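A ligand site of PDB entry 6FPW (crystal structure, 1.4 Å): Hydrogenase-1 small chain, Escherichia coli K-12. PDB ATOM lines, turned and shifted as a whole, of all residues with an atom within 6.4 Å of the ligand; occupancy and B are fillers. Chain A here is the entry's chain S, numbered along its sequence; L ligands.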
ATOM      1  N   ILE A 186      -9.322  18.073 -27.460  1.00  0.00           N
ATOM      2  CA  ILE A 186      -9.220  18.951 -26.293  1.00  0.00           C
ATOM      3  C   ILE A 186     -10.584  19.122 -25.634  1.00  0.00           C
ATOM      4  O   ILE A 186     -10.764  18.986 -24.409  1.00  0.00           O
ATOM      5  CB  ILE A 186      -8.662  20.328 -26.706  1.00  0.00           C
ATOM      6  CG1 ILE A 186      -7.199  20.240 -27.156  1.00  0.00           C
ATOM      7  CG2 ILE A 186      -8.829  21.367 -25.613  1.00  0.00           C
ATOM      8  CD1 ILE A 186      -6.242  19.728 -26.131  1.00  0.00           C
ATOM      9  N   HIS A 187     -11.587  19.381 -26.464  1.00  0.00           N
ATOM     10  CA  HIS A 187     -12.979  19.650 -26.032  1.00  0.00           C
ATOM     11  C   HIS A 187     -13.670  18.430 -25.416  1.00  0.00           C
ATOM     12  O   HIS A 187     -14.675  18.590 -24.730  1.00  0.00           O
ATOM     13  CB  HIS A 187     -13.704  20.139 -27.276  1.00  0.00           C
ATOM     14  CG  HIS A 187     -15.137  20.533 -27.168  1.00  0.00           C
ATOM     15  ND1 HIS A 187     -15.588  21.689 -26.564  1.00  0.00           N
ATOM     16  CD2 HIS A 187     -16.236  19.943 -27.728  1.00  0.00           C
ATOM     17  CE1 HIS A 187     -16.909  21.780 -26.734  1.00  0.00           C
ATOM     18  NE2 HIS A 187     -17.323  20.753 -27.464  1.00  0.00           N
ATOM     19  N   ASP A 188     -13.156  17.245 -25.701  1.00  0.00           N
ATOM     20  CA  ASP A 188     -13.703  15.971 -25.155  1.00  0.00           C
ATOM     21  C   ASP A 188     -13.233  15.749 -23.697  1.00  0.00           C
ATOM     22  O   ASP A 188     -13.736  14.820 -23.023  1.00  0.00           O
ATOM     23  CB  ASP A 188     -13.187  14.712 -25.954  1.00  0.00           C
ATOM     24  CG  ASP A 188     -13.562  14.587 -27.435  1.00  0.00           C
ATOM     25  OD1 ASP A 188     -14.602  15.114 -27.807  1.00  0.00           O
ATOM     26  OD2 ASP A 188     -12.740  13.829 -28.209  1.00  0.00           O
ATOM     27  N   CYS A 190     -12.289  18.739 -21.670  1.00  0.00           N
ATOM     28  CA  CYS A 190     -12.089  20.123 -21.161  1.00  0.00           C
ATOM     29  C   CYS A 190     -12.909  20.388 -19.916  1.00  0.00           C
ATOM     30  O   CYS A 190     -14.124  20.158 -19.906  1.00  0.00           O
ATOM     31  CB  CYS A 190     -12.452  21.130 -22.244  1.00  0.00           C
ATOM     32  SG  CYS A 190     -12.140  22.838 -21.717  1.00  0.00           S
ATOM     33  N   TYR A 191     -12.245  20.893 -18.895  1.00  0.00           N
ATOM     34  CA  TYR A 191     -12.935  21.204 -17.633  1.00  0.00           C
ATOM     35  C   TYR A 191     -13.957  22.316 -17.734  1.00  0.00           C
ATOM     36  O   TYR A 191     -14.705  22.485 -16.796  1.00  0.00           O
ATOM     37  CB  TYR A 191     -11.890  21.420 -16.477  1.00  0.00           C
ATOM     38  CG  TYR A 191     -11.313  22.832 -16.409  1.00  0.00           C
ATOM     39  CD1 TYR A 191     -10.695  23.468 -17.484  1.00  0.00           C
ATOM     40  CD2 TYR A 191     -11.422  23.560 -15.245  1.00  0.00           C
ATOM     41  CE1 TYR A 191     -10.216  24.740 -17.379  1.00  0.00           C
ATOM     42  CE2 TYR A 191     -10.913  24.839 -15.136  1.00  0.00           C
ATOM     43  CZ  TYR A 191     -10.365  25.458 -16.224  1.00  0.00           C
ATOM     44  OH  TYR A 191      -9.942  26.760 -16.128  1.00  0.00           O
ATOM     45  N   ARG A 192     -13.996  23.050 -18.851  1.00  0.00           N
ATOM     46  CA  ARG A 192     -15.049  24.050 -19.039  1.00  0.00           C
ATOM     47  C   ARG A 192     -16.241  23.557 -19.853  1.00  0.00           C
ATOM     48  O   ARG A 192     -17.148  24.321 -20.156  1.00  0.00           O
ATOM     49  CB  ARG A 192     -14.435  25.306 -19.670  1.00  0.00           C
ATOM     50  CG  ARG A 192     -13.365  25.971 -18.794  1.00  0.00           C
ATOM     51  CD  ARG A 192     -12.892  27.304 -19.321  1.00  0.00           C
ATOM     52  NE  ARG A 192     -11.853  27.840 -18.481  1.00  0.00           N
ATOM     53  CZ  ARG A 192     -11.501  29.114 -18.369  1.00  0.00           C
ATOM     54  NH1 ARG A 192     -12.154  30.049 -18.994  1.00  0.00           N
ATOM     55  NH2 ARG A 192     -10.479  29.443 -17.547  1.00  0.00           N
ATOM     56  N   ARG A 193     -16.283  22.262 -20.115  1.00  0.00           N
ATOM     57  CA  ARG A 193     -17.357  21.704 -20.921  1.00  0.00           C
ATOM     58  C   ARG A 193     -18.725  21.874 -20.299  1.00  0.00           C
ATOM     59  O   ARG A 193     -19.705  22.085 -21.024  1.00  0.00           O
ATOM     60  CB  ARG A 193     -17.100  20.240 -21.193  1.00  0.00           C
ATOM     61  CG  ARG A 193     -17.944  19.636 -22.182  1.00  0.00           C
ATOM     62  CD  ARG A 193     -17.832  20.250 -23.596  1.00  0.00           C
ATOM     63  NE  ARG A 193     -18.893  19.551 -24.225  1.00  0.00           N
ATOM     64  CZ  ARG A 193     -18.771  18.498 -25.014  1.00  0.00           C
ATOM     65  NH1 ARG A 193     -17.616  18.008 -25.422  1.00  0.00           N
ATOM     66  NH2 ARG A 193     -19.884  17.952 -25.419  1.00  0.00           N
ATOM     67  N   ALA A 194     -18.819  21.837 -18.959  1.00  0.00           N
ATOM     68  CA  ALA A 194     -20.073  22.095 -18.297  1.00  0.00           C
ATOM     69  C   ALA A 194     -20.645  23.423 -18.746  1.00  0.00           C
ATOM     70  O   ALA A 194     -21.876  23.570 -18.935  1.00  0.00           O
ATOM     71  CB  ALA A 194     -19.887  22.146 -16.799  1.00  0.00           C
ATOM     72  N   HIS A 195     -19.789  24.426 -18.875  1.00  0.00           N
ATOM     73  CA  HIS A 195     -20.247  25.763 -19.308  1.00  0.00           C
ATOM     74  C   HIS A 195     -20.657  25.801 -20.788  1.00  0.00           C
ATOM     75  O   HIS A 195     -21.679  26.375 -21.120  1.00  0.00           O
ATOM     76  CB  HIS A 195     -19.143  26.773 -19.025  1.00  0.00           C
ATOM     77  CG  HIS A 195     -18.779  26.840 -17.574  1.00  0.00           C
ATOM     78  ND1 HIS A 195     -19.708  27.114 -16.594  1.00  0.00           N
ATOM     79  CD2 HIS A 195     -17.579  26.724 -16.938  1.00  0.00           C
ATOM     80  CE1 HIS A 195     -19.095  27.136 -15.412  1.00  0.00           C
ATOM     81  NE2 HIS A 195     -17.800  26.920 -15.592  1.00  0.00           N
ATOM     82  N   PHE A 196     -19.901  25.124 -21.635  1.00  0.00           N
ATOM     83  CA  PHE A 196     -20.281  25.000 -23.059  1.00  0.00           C
ATOM     84  C   PHE A 196     -21.672  24.380 -23.192  1.00  0.00           C
ATOM     85  O   PHE A 196     -22.532  24.935 -23.852  1.00  0.00           O
ATOM     86  CB  PHE A 196     -19.261  24.129 -23.767  1.00  0.00           C
ATOM     87  CG  PHE A 196     -19.579  23.848 -25.224  1.00  0.00           C
ATOM     88  CD1 PHE A 196     -19.129  24.725 -26.189  1.00  0.00           C
ATOM     89  CD2 PHE A 196     -20.297  22.720 -25.622  1.00  0.00           C
ATOM     90  CE1 PHE A 196     -19.417  24.512 -27.521  1.00  0.00           C
ATOM     91  CE2 PHE A 196     -20.535  22.466 -26.951  1.00  0.00           C
ATOM     92  CZ  PHE A 196     -20.103  23.356 -27.907  1.00  0.00           C
ATOM     93  N   PHE A 201     -20.837  31.357 -21.618  1.00  0.00           N
ATOM     94  CA  PHE A 201     -19.696  31.740 -22.471  1.00  0.00           C
ATOM     95  C   PHE A 201     -19.126  33.076 -22.040  1.00  0.00           C
ATOM     96  O   PHE A 201     -19.846  34.044 -21.751  1.00  0.00           O
ATOM     97  CB  PHE A 201     -20.113  31.848 -23.935  1.00  0.00           C
ATOM     98  CG  PHE A 201     -20.665  30.577 -24.516  1.00  0.00           C
ATOM     99  CD1 PHE A 201     -19.836  29.523 -24.705  1.00  0.00           C
ATOM    100  CD2 PHE A 201     -22.027  30.483 -24.892  1.00  0.00           C
ATOM    101  CE1 PHE A 201     -20.335  28.340 -25.236  1.00  0.00           C
ATOM    102  CE2 PHE A 201     -22.494  29.350 -25.482  1.00  0.00           C
ATOM    103  CZ  PHE A 201     -21.670  28.252 -25.645  1.00  0.00           C
ATOM    104  N   TYR A 214     -15.811  30.604 -17.488  1.00  0.00           N
ATOM    105  CA  TYR A 214     -16.754  30.110 -18.469  1.00  0.00           C
ATOM    106  C   TYR A 214     -16.039  29.749 -19.789  1.00  0.00           C
ATOM    107  O   TYR A 214     -14.846  29.992 -19.991  1.00  0.00           O
ATOM    108  CB  TYR A 214     -17.875  31.135 -18.732  1.00  0.00           C
ATOM    109  CG  TYR A 214     -18.960  31.209 -17.649  1.00  0.00           C
ATOM    110  CD1 TYR A 214     -18.857  30.538 -16.430  1.00  0.00           C
ATOM    111  CD2 TYR A 214     -20.120  31.962 -17.887  1.00  0.00           C
ATOM    112  CE1 TYR A 214     -19.869  30.623 -15.452  1.00  0.00           C
ATOM    113  CE2 TYR A 214     -21.129  32.020 -16.955  1.00  0.00           C
ATOM    114  CZ  TYR A 214     -20.968  31.387 -15.730  1.00  0.00           C
ATOM    115  OH  TYR A 214     -21.980  31.457 -14.771  1.00  0.00           O
ATOM    116  N   CYS A 215     -16.789  29.059 -20.625  1.00  0.00           N
ATOM    117  CA  CYS A 215     -16.284  28.464 -21.857  1.00  0.00           C
ATOM    118  C   CYS A 215     -15.875  29.556 -22.849  1.00  0.00           C
ATOM    119  O   CYS A 215     -16.487  30.653 -22.890  1.00  0.00           O
ATOM    120  CB  CYS A 215     -17.323  27.522 -22.458  1.00  0.00           C
ATOM    121  SG  CYS A 215     -16.999  27.007 -24.175  1.00  0.00           S
ATOM    122  N   LEU A 216     -14.810  29.260 -23.571  1.00  0.00           N
ATOM    123  CA  LEU A 216     -14.145  30.183 -24.508  1.00  0.00           C
ATOM    124  C   LEU A 216     -14.565  29.993 -25.967  1.00  0.00           C
ATOM    125  O   LEU A 216     -13.985  30.640 -26.876  1.00  0.00           O
ATOM    126  CB  LEU A 216     -12.622  30.088 -24.338  1.00  0.00           C
ATOM    127  CG  LEU A 216     -12.192  30.450 -22.927  1.00  0.00           C
ATOM    128  CD1 LEU A 216     -10.730  30.092 -22.713  1.00  0.00           C
ATOM    129  CD2 LEU A 216     -12.362  31.901 -22.600  1.00  0.00           C
ATOM    130  N   TYR A 217     -15.600  29.217 -26.233  1.00  0.00           N
ATOM    131  CA  TYR A 217     -16.054  28.950 -27.623  1.00  0.00           C
ATOM    132  C   TYR A 217     -16.352  30.245 -28.418  1.00  0.00           C
ATOM    133  O   TYR A 217     -15.930  30.385 -29.565  1.00  0.00           O
ATOM    134  CB  TYR A 217     -17.312  28.072 -27.511  1.00  0.00           C
ATOM    135  CG  TYR A 217     -18.016  27.939 -28.840  1.00  0.00           C
ATOM    136  CD1 TYR A 217     -17.461  27.172 -29.870  1.00  0.00           C
ATOM    137  CD2 TYR A 217     -19.218  28.609 -29.063  1.00  0.00           C
ATOM    138  CE1 TYR A 217     -18.092  27.101 -31.117  1.00  0.00           C
ATOM    139  CE2 TYR A 217     -19.831  28.542 -30.276  1.00  0.00           C
ATOM    140  CZ  TYR A 217     -19.276  27.792 -31.287  1.00  0.00           C
ATOM    141  OH  TYR A 217     -19.966  27.777 -32.427  1.00  0.00           O
ATOM    142  N   LYS A 218     -17.024  31.190 -27.779  1.00  0.00           N
ATOM    143  CA  LYS A 218     -17.374  32.438 -28.477  1.00  0.00           C
ATOM    144  C   LYS A 218     -16.212  33.370 -28.639  1.00  0.00           C
ATOM    145  O   LYS A 218     -16.280  34.306 -29.430  1.00  0.00           O
ATOM    146  CB  LYS A 218     -18.577  33.158 -27.809  1.00  0.00           C
ATOM    147  CG  LYS A 218     -19.878  32.348 -27.884  1.00  0.00           C
ATOM    148  CD  LYS A 218     -21.096  33.185 -27.521  1.00  0.00           C
ATOM    149  CE  LYS A 218     -22.323  32.367 -27.839  1.00  0.00           C
ATOM    150  NZ  LYS A 218     -23.543  33.087 -27.390  1.00  0.00           N
ATOM    151  N   CYS A 221     -12.257  29.590 -29.341  1.00  0.00           N
ATOM    152  CA  CYS A 221     -11.579  28.346 -28.951  1.00  0.00           C
ATOM    153  C   CYS A 221     -11.717  27.259 -29.981  1.00  0.00           C
ATOM    154  O   CYS A 221     -12.826  26.951 -30.442  1.00  0.00           O
ATOM    155  CB  CYS A 221     -12.176  27.822 -27.629  1.00  0.00           C
ATOM    156  SG  CYS A 221     -11.310  26.386 -27.012  1.00  0.00           S
ATOM    157  N   LYS A 222     -10.591  26.710 -30.404  1.00  0.00           N
ATOM    158  CA  LYS A 222     -10.539  25.630 -31.411  1.00  0.00           C
ATOM    159  C   LYS A 222     -10.465  24.248 -30.795  1.00  0.00           C
ATOM    160  O   LYS A 222     -10.258  23.252 -31.476  1.00  0.00           O
ATOM    161  CB  LYS A 222      -9.405  25.886 -32.418  1.00  0.00           C
ATOM    162  CG  LYS A 222      -9.584  27.231 -33.153  1.00  0.00           C
ATOM    163  CD  LYS A 222     -10.968  27.356 -33.757  1.00  0.00           C
ATOM    164  CE  LYS A 222     -11.340  28.569 -34.538  1.00  0.00           C
ATOM    165  NZ  LYS A 222     -10.794  29.844 -34.110  1.00  0.00           N
ATOM    166  N   GLY A 223     -10.676  24.149 -29.472  1.00  0.00           N
ATOM    167  CA  GLY A 223     -10.699  22.851 -28.800  1.00  0.00           C
ATOM    168  C   GLY A 223     -11.619  21.797 -29.449  1.00  0.00           C
ATOM    169  O   GLY A 223     -11.248  20.632 -29.491  1.00  0.00           O
ATOM    170  N   PRO A 224     -12.802  22.227 -29.960  1.00  0.00           N
ATOM    171  CA  PRO A 224     -13.700  21.265 -30.569  1.00  0.00           C
ATOM    172  C   PRO A 224     -13.159  20.534 -31.789  1.00  0.00           C
ATOM    173  O   PRO A 224     -13.703  19.482 -32.127  1.00  0.00           O
ATOM    174  CB  PRO A 224     -14.892  22.094 -30.904  1.00  0.00           C
ATOM    175  CG  PRO A 224     -14.942  23.198 -29.933  1.00  0.00           C
ATOM    176  CD  PRO A 224     -13.489  23.536 -29.749  1.00  0.00           C
ATOM    177  N   PHE A 241      -3.002  25.030 -18.897  1.00  0.00           N
ATOM    178  CA  PHE A 241      -3.020  24.882 -20.345  1.00  0.00           C
ATOM    179  C   PHE A 241      -3.691  26.123 -20.886  1.00  0.00           C
ATOM    180  O   PHE A 241      -4.238  26.945 -20.121  1.00  0.00           O
ATOM    181  CB  PHE A 241      -3.652  23.552 -20.787  1.00  0.00           C
ATOM    182  CG  PHE A 241      -5.146  23.406 -20.690  1.00  0.00           C
ATOM    183  CD1 PHE A 241      -5.801  23.326 -19.473  1.00  0.00           C
ATOM    184  CD2 PHE A 241      -5.880  23.244 -21.856  1.00  0.00           C
ATOM    185  CE1 PHE A 241      -7.182  23.085 -19.418  1.00  0.00           C
ATOM    186  CE2 PHE A 241      -7.248  23.037 -21.792  1.00  0.00           C
ATOM    187  CZ  PHE A 241      -7.878  22.967 -20.584  1.00  0.00           C
ATOM    188  N   ILE A 243      -6.506  27.113 -22.224  1.00  0.00           N
ATOM    189  CA  ILE A 243      -7.866  27.399 -21.817  1.00  0.00           C
ATOM    190  C   ILE A 243      -7.929  27.704 -20.321  1.00  0.00           C
ATOM    191  O   ILE A 243      -8.659  28.627 -19.903  1.00  0.00           O
ATOM    192  CB  ILE A 243      -8.785  26.244 -22.253  1.00  0.00           C
ATOM    193  CG1 ILE A 243      -9.019  26.258 -23.765  1.00  0.00           C
ATOM    194  CG2 ILE A 243     -10.109  26.204 -21.450  1.00  0.00           C
ATOM    195  CD1 ILE A 243      -9.234  24.879 -24.337  1.00  0.00           C
ATOM    196  N   GLY A 248      -8.657  30.828 -25.600  1.00  0.00           N
ATOM    197  CA  GLY A 248      -9.079  29.640 -26.313  1.00  0.00           C
ATOM    198  C   GLY A 248      -7.898  28.913 -26.912  1.00  0.00           C
ATOM    199  O   GLY A 248      -6.878  29.502 -27.300  1.00  0.00           O
ATOM    200  N   CYS A 249      -8.065  27.629 -27.127  1.00  0.00           N
ATOM    201  CA  CYS A 249      -7.163  26.840 -27.964  1.00  0.00           C
ATOM    202  C   CYS A 249      -7.047  27.489 -29.348  1.00  0.00           C
ATOM    203  O   CYS A 249      -8.072  27.905 -29.905  1.00  0.00           O
ATOM    204  CB  CYS A 249      -7.697  25.393 -28.018  1.00  0.00           C
ATOM    205  SG  CYS A 249      -6.784  24.218 -29.107  1.00  0.00           S
HETATM  206 FE1  LIG L   1     -15.250  25.552 -24.291  1.00  0.00          FE
HETATM  207 FE2  LIG L   1     -12.902  25.368 -25.706  1.00  0.00          FE
HETATM  208 FE3  LIG L   1     -14.650  23.267 -25.624  1.00  0.00          FE
HETATM  209 FE4  LIG L   1     -13.235  23.910 -23.416  1.00  0.00          FE
HETATM  210  S1  LIG L   1     -12.383  23.137 -25.429  1.00  0.00           S
HETATM  211  S2  LIG L   1     -15.476  23.411 -23.473  1.00  0.00           S
HETATM  212  S3  LIG L   1     -13.184  26.214 -23.552  1.00  0.00           S
HETATM  213  S4  LIG L   1     -15.001  25.295 -26.604  1.00  0.00           S
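The guanidinium group (NH1) of Arg 192 lies within hydrogen-bond range of the backbone carbonyl oxygen (O) of Tyr 214. NH2 of Arg 192 lies within hydrogen-bond range of O of Ile 243 (3.1 Å). The backbone NH (N) of Tyr 217 lies close to the side-chain sulfur (SG) of Cys 215 (3.3 Å). The backbone NH (N) of Arg 192 sits close to the side-chain sulfur (SG) of Cys 190 (3.4 Å). N of Cys 221 lies within hydrogen-bond range of O of Leu 216 (3.2 Å). The backbone NH of His 187 lies within hydrogen-bond range of the backbone carbonyl oxygen of Gly 223 (3.3 Å). NH2 of Arg 192 lies within hydrogen-bond range of OH of Tyr 191, 3.1 Å away. The backbone carbonyl oxygen (O) of His 187 sits at hydrogen-bond distance from the guanidinium group (NH1) of Arg 193 (3.1 Å).
An iron atom (FE3) of the ligand is bound by a ring nitrogen (ND1) of His 187 (2.1 Å). SG of Cys 215 binds FE1 of the ligand (2.3 Å). The side-chain sulfur of Cys 190 binds an iron atom (FE4) of the ligand (2.3 Å). A sulfur (S3) of the ligand sits close to the backbone NH of Leu 216 (3.5 Å). An iron atom (FE2) of the ligand is bound by the side-chain sulfur of Cys 221 (2.3 Å). N of Arg 193 sits close to S2 of the ligand, at 3.6 Å.
Residues that only touch the ligand: Ile 186, Arg 192, Phe 196, Tyr 217, Gly 223, Pro 224 and Ile 243. Hydrophobic or aromatic side chains within 4 Å of the ligand: Ile 186, His 187, Phe 196, Leu 216, Tyr 217, Pro 224 and Ile 243. Of the 24 residues printed, 13 come within 4 Å of the ligand.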
